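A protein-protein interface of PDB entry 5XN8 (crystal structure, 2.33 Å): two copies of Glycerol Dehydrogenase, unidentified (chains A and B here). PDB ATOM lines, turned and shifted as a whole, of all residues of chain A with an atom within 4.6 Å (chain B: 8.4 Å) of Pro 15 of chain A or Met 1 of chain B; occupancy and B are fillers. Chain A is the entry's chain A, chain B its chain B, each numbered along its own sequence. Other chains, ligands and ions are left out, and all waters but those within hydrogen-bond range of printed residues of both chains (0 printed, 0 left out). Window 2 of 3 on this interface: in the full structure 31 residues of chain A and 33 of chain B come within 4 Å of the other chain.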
ATOM      1  N   GLN A  13       2.606  27.300  30.147  1.00  0.00           N
ATOM      2  CA  GLN A  13       3.165  27.966  31.323  1.00  0.00           C
ATOM      3  C   GLN A  13       4.678  28.131  31.270  1.00  0.00           C
ATOM      4  O   GLN A  13       5.391  27.174  31.059  1.00  0.00           O
ATOM      5  CB  GLN A  13       2.789  27.198  32.586  1.00  0.00           C
ATOM      6  CG  GLN A  13       3.286  27.854  33.864  1.00  0.00           C
ATOM      7  CD  GLN A  13       3.107  26.951  35.054  1.00  0.00           C
ATOM      8  OE1 GLN A  13       2.005  26.463  35.305  1.00  0.00           O
ATOM      9  NE2 GLN A  13       4.200  26.680  35.776  1.00  0.00           N
ATOM     10  N   GLY A  14       5.146  29.350  31.520  1.00  0.00           N
ATOM     11  CA  GLY A  14       6.580  29.637  31.600  1.00  0.00           C
ATOM     12  C   GLY A  14       6.879  31.118  31.469  1.00  0.00           C
ATOM     13  O   GLY A  14       5.962  31.930  31.322  1.00  0.00           O
ATOM     14  N   PRO A  15       8.166  31.488  31.523  1.00  0.00           N
ATOM     15  CA  PRO A  15       8.566  32.870  31.230  1.00  0.00           C
ATOM     16  C   PRO A  15       8.161  33.285  29.819  1.00  0.00           C
ATOM     17  O   PRO A  15       8.321  32.500  28.887  1.00  0.00           O
ATOM     18  CB  PRO A  15      10.093  32.824  31.362  1.00  0.00           C
ATOM     19  CG  PRO A  15      10.343  31.738  32.342  1.00  0.00           C
ATOM     20  CD  PRO A  15       9.286  30.698  32.064  1.00  0.00           C
ATOM     21  N   ASP A  16       7.613  34.491  29.687  1.00  0.00           N
ATOM     22  CA  ASP A  16       7.246  35.078  28.384  1.00  0.00           C
ATOM     23  C   ASP A  16       6.194  34.277  27.592  1.00  0.00           C
ATOM     24  O   ASP A  16       6.138  34.370  26.375  1.00  0.00           O
ATOM     25  CB  ASP A  16       8.495  35.313  27.528  1.00  0.00           C
ATOM     26  CG  ASP A  16       9.556  36.129  28.254  1.00  0.00           C
ATOM     27  OD1 ASP A  16       9.255  37.255  28.716  1.00  0.00           O
ATOM     28  OD2 ASP A  16      10.701  35.640  28.378  1.00  0.00           O
ATOM     29  N   ALA A  17       5.341  33.525  28.283  1.00  0.00           N
ATOM     30  CA  ALA A  17       4.299  32.734  27.626  1.00  0.00           C
ATOM     31  C   ALA A  17       3.265  33.587  26.890  1.00  0.00           C
ATOM     32  O   ALA A  17       2.679  33.131  25.909  1.00  0.00           O
ATOM     33  CB  ALA A  17       3.610  31.820  28.627  1.00  0.00           C
ATOM     34  N   LEU A  20       4.741  34.054  23.485  1.00  0.00           N
ATOM     35  CA  LEU A  20       5.117  32.808  22.807  1.00  0.00           C
ATOM     36  C   LEU A  20       3.940  31.902  22.412  1.00  0.00           C
ATOM     37  O   LEU A  20       4.149  30.900  21.722  1.00  0.00           O
ATOM     38  CB  LEU A  20       6.082  32.009  23.700  1.00  0.00           C
ATOM     39  CG  LEU A  20       7.477  32.590  23.914  1.00  0.00           C
ATOM     40  CD1 LEU A  20       8.209  31.774  24.974  1.00  0.00           C
ATOM     41  CD2 LEU A  20       8.271  32.628  22.614  1.00  0.00           C
ATOM     42  N   ASP A 153       1.845  33.333  31.986  1.00  0.00           N
ATOM     43  CA  ASP A 153       3.149  33.975  31.908  1.00  0.00           C
ATOM     44  C   ASP A 153       3.618  34.220  33.328  1.00  0.00           C
ATOM     45  O   ASP A 153       3.148  35.147  34.003  1.00  0.00           O
ATOM     46  CB  ASP A 153       3.096  35.290  31.111  1.00  0.00           C
ATOM     47  CG  ASP A 153       4.491  35.832  30.784  1.00  0.00           C
ATOM     48  OD1 ASP A 153       5.430  35.623  31.580  1.00  0.00           O
ATOM     49  OD2 ASP A 153       4.650  36.456  29.721  1.00  0.00           O
ATOM     50  N   THR A 154       4.560  33.391  33.767  1.00  0.00           N
ATOM     51  CA  THR A 154       5.009  33.393  35.156  1.00  0.00           C
ATOM     52  C   THR A 154       5.929  34.571  35.494  1.00  0.00           C
ATOM     53  O   THR A 154       6.148  34.846  36.665  1.00  0.00           O
ATOM     54  CB  THR A 154       5.735  32.075  35.481  1.00  0.00           C
ATOM     55  OG1 THR A 154       6.863  31.937  34.614  1.00  0.00           O
ATOM     56  CG2 THR A 154       4.787  30.878  35.291  1.00  0.00           C
ATOM     57  N   ALA A 155       6.477  35.245  34.482  1.00  0.00           N
ATOM     58  CA  ALA A 155       7.223  36.497  34.685  1.00  0.00           C
ATOM     59  C   ALA A 155       6.284  37.636  35.071  1.00  0.00           C
ATOM     60  O   ALA A 155       6.633  38.485  35.898  1.00  0.00           O
ATOM     61  CB  ALA A 155       8.020  36.859  33.432  1.00  0.00           C
ATOM     62  N   GLU A 231       6.819  28.088  39.780  1.00  0.00           N
ATOM     63  CA  GLU A 231       6.263  27.412  38.602  1.00  0.00           C
ATOM     64  C   GLU A 231       5.382  26.240  39.032  1.00  0.00           C
ATOM     65  O   GLU A 231       4.305  26.060  38.479  1.00  0.00           O
ATOM     66  CB  GLU A 231       7.384  26.905  37.671  1.00  0.00           C
ATOM     67  CG  GLU A 231       8.228  27.993  37.007  1.00  0.00           C
ATOM     68  CD  GLU A 231       7.638  28.578  35.724  1.00  0.00           C
ATOM     69  OE1 GLU A 231       6.836  27.907  35.051  1.00  0.00           O
ATOM     70  OE2 GLU A 231       8.011  29.718  35.368  1.00  0.00           O
ATOM     71  N   MET B   1      11.225  27.233  26.588  1.00  0.00           N
ATOM     72  CA  MET B   1      11.090  26.903  28.035  1.00  0.00           C
ATOM     73  C   MET B   1       9.650  27.019  28.558  1.00  0.00           C
ATOM     74  O   MET B   1       9.456  27.243  29.756  1.00  0.00           O
ATOM     75  CB  MET B   1      12.044  27.794  28.881  1.00  0.00           C
ATOM     76  CG  MET B   1      12.283  27.309  30.323  1.00  0.00           C
ATOM     77  SD  MET B   1      12.091  28.573  31.627  1.00  0.00           S
ATOM     78  CE  MET B   1      11.459  27.597  33.000  1.00  0.00           C
ATOM     79  N   LEU B   2       8.646  26.840  27.693  1.00  0.00           N
ATOM     80  CA  LEU B   2       7.259  26.688  28.139  1.00  0.00           C
ATOM     81  C   LEU B   2       7.000  25.237  28.543  1.00  0.00           C
ATOM     82  O   LEU B   2       7.539  24.307  27.930  1.00  0.00           O
ATOM     83  CB  LEU B   2       6.274  27.066  27.035  1.00  0.00           C
ATOM     84  CG  LEU B   2       6.353  28.471  26.455  1.00  0.00           C
ATOM     85  CD1 LEU B   2       5.444  28.584  25.240  1.00  0.00           C
ATOM     86  CD2 LEU B   2       5.985  29.482  27.521  1.00  0.00           C
ATOM     87  N   LYS B   3       6.176  25.052  29.580  1.00  0.00           N
ATOM     88  CA  LYS B   3       5.621  23.744  29.900  1.00  0.00           C
ATOM     89  C   LYS B   3       4.275  23.661  29.196  1.00  0.00           C
ATOM     90  O   LYS B   3       3.505  24.626  29.215  1.00  0.00           O
ATOM     91  CB  LYS B   3       5.467  23.561  31.405  1.00  0.00           C
ATOM     92  CG  LYS B   3       6.802  23.467  32.135  1.00  0.00           C
ATOM     93  CD  LYS B   3       6.661  23.525  33.650  1.00  0.00           C
ATOM     94  CE  LYS B   3       6.052  24.844  34.124  1.00  0.00           C
ATOM     95  NZ  LYS B   3       6.574  26.058  33.425  1.00  0.00           N
ATOM     96  N   VAL B   4       4.004  22.530  28.546  1.00  0.00           N
ATOM     97  CA  VAL B   4       2.737  22.352  27.825  1.00  0.00           C
ATOM     98  C   VAL B   4       2.127  21.009  28.174  1.00  0.00           C
ATOM     99  O   VAL B   4       2.837  20.019  28.303  1.00  0.00           O
ATOM    100  CB  VAL B   4       2.898  22.471  26.292  1.00  0.00           C
ATOM    101  CG1 VAL B   4       1.533  22.544  25.610  1.00  0.00           C
ATOM    102  CG2 VAL B   4       3.707  23.706  25.930  1.00  0.00           C
ATOM    103  N   ARG B 186      15.149  16.660  29.905  1.00  0.00           N
ATOM    104  CA  ARG B 186      14.593  17.953  29.495  1.00  0.00           C
ATOM    105  C   ARG B 186      14.274  17.924  27.999  1.00  0.00           C
ATOM    106  O   ARG B 186      14.569  18.866  27.260  1.00  0.00           O
ATOM    107  CB  ARG B 186      15.524  19.124  29.875  1.00  0.00           C
ATOM    108  CG  ARG B 186      16.113  19.070  31.289  1.00  0.00           C
ATOM    109  CD  ARG B 186      15.258  19.735  32.343  1.00  0.00           C
ATOM    110  NE  ARG B 186      13.888  19.220  32.330  1.00  0.00           N
ATOM    111  CZ  ARG B 186      12.776  19.907  32.612  1.00  0.00           C
ATOM    112  NH1 ARG B 186      12.798  21.197  32.936  1.00  0.00           N
ATOM    113  NH2 ARG B 186      11.595  19.279  32.550  1.00  0.00           N
ATOM    114  N   THR B 188      11.746  17.710  24.700  1.00  0.00           N
ATOM    115  CA  THR B 188      10.461  18.235  24.252  1.00  0.00           C
ATOM    116  C   THR B 188       9.490  17.105  23.898  1.00  0.00           C
ATOM    117  O   THR B 188       9.894  16.102  23.302  1.00  0.00           O
ATOM    118  CB  THR B 188      10.665  19.137  23.024  1.00  0.00           C
ATOM    119  OG1 THR B 188      11.595  20.173  23.365  1.00  0.00           O
ATOM    120  CG2 THR B 188       9.374  19.786  22.559  1.00  0.00           C
ATOM    121  N   GLY B 192       4.688  20.098  22.772  1.00  0.00           N
ATOM    122  CA  GLY B 192       5.544  21.141  22.213  1.00  0.00           C
ATOM    123  C   GLY B 192       6.548  21.782  23.163  1.00  0.00           C
ATOM    124  O   GLY B 192       7.342  22.617  22.726  1.00  0.00           O
ATOM    125  N   GLY B 193       6.518  21.407  24.446  1.00  0.00           N
ATOM    126  CA  GLY B 193       7.452  21.962  25.439  1.00  0.00           C
ATOM    127  C   GLY B 193       7.942  20.929  26.433  1.00  0.00           C
ATOM    128  O   GLY B 193       7.926  19.716  26.161  1.00  0.00           O
ATOM    129  N   GLN B 194       8.395  21.407  27.585  1.00  0.00           N
ATOM    130  CA  GLN B 194       8.793  20.525  28.683  1.00  0.00           C
ATOM    131  C   GLN B 194       7.544  19.921  29.336  1.00  0.00           C
ATOM    132  O   GLN B 194       6.418  20.361  29.070  1.00  0.00           O
ATOM    133  CB  GLN B 194       9.597  21.293  29.740  1.00  0.00           C
ATOM    134  CG  GLN B 194      10.845  22.014  29.231  1.00  0.00           C
ATOM    135  CD  GLN B 194      11.872  21.087  28.631  1.00  0.00           C
ATOM    136  OE1 GLN B 194      11.974  19.926  29.012  1.00  0.00           O
ATOM    137  NE2 GLN B 194      12.665  21.605  27.708  1.00  0.00           N
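Among the printed residues, merely in contact across the chains: Gln 13 of chain A with Leu 2 of chain B (3.5 Å), Ala 17 of chain A with Leu 2 of chain B (3.5 Å), Pro 15 of chain A with Met 1 of chain B (3.5 Å) and Leu 20 of chain A with Leu 2 of chain B (3.8 Å).
The backbone NH of Lys 3 of chain B sits at hydrogen-bond distance from the backbone carbonyl oxygen of Gln 13 of chain A, 2.7 Å away. OE1 of Glu 231 of chain A lies within salt-bridge range of NZ of Lys 3 of chain B (2.5 Å).
NE2 of Gln 13 of chain A sits at hydrogen-bond distance from O of Glu 231 of chain A (2.8 Å). N of Ala 17 of chain A is in hydrogen-bond range of OD2 of Asp 153 of chain A (3.3 Å). OE2 of Glu 231 of chain A sits at hydrogen-bond distance from OG1 of Thr 154 of chain A (2.6 Å). The backbone carbonyl oxygen (O) of Leu 2 of chain B is in hydrogen-bond range of the backbone NH (N) of Gln 194 of chain B (3.0 Å).
No position is printed for both chains. Of the 6 pairs that touch across the chains among the printed residues, none has its exchanged pair printed and touching as well.
Printed residues of chain B within 4 Å of Gln 13 of chain A: Leu 2 and Lys 3. Pro 15 of chain A touches just one residue of chain B: Met 1 (3.5 Å). Of the printed residues of chain B, Ala 17 of chain A touches Leu 2 (3.5 Å). Of the printed residues of chain B, Leu 20 of chain A touches Leu 2 (3.8 Å). Of chain A, only Pro 15 (3.5 Å) comes within 4 Å of Met 1 of chain B. Of the printed residues of chain A, Leu 2 of chain B touches Gln 13 (3.5 Å), Ala 17 (3.5 Å) and Leu 20 (3.8 Å). Printed residues of chain A within 4 Å of Lys 3 of chain B: Gln 13 (2.7 Å) and Glu 231 (2.5 Å). The nearest residue of chain A that does not touch Met 1 of chain B is Gly 14 of chain A (4.2 Å).
Among the printed residues, Asp or Glu carboxylates within 4 Å of a Lys or Arg side-chain nitrogen of the other chain: Glu 231 of chain A with Lys 3 of chain B (2.5 Å).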
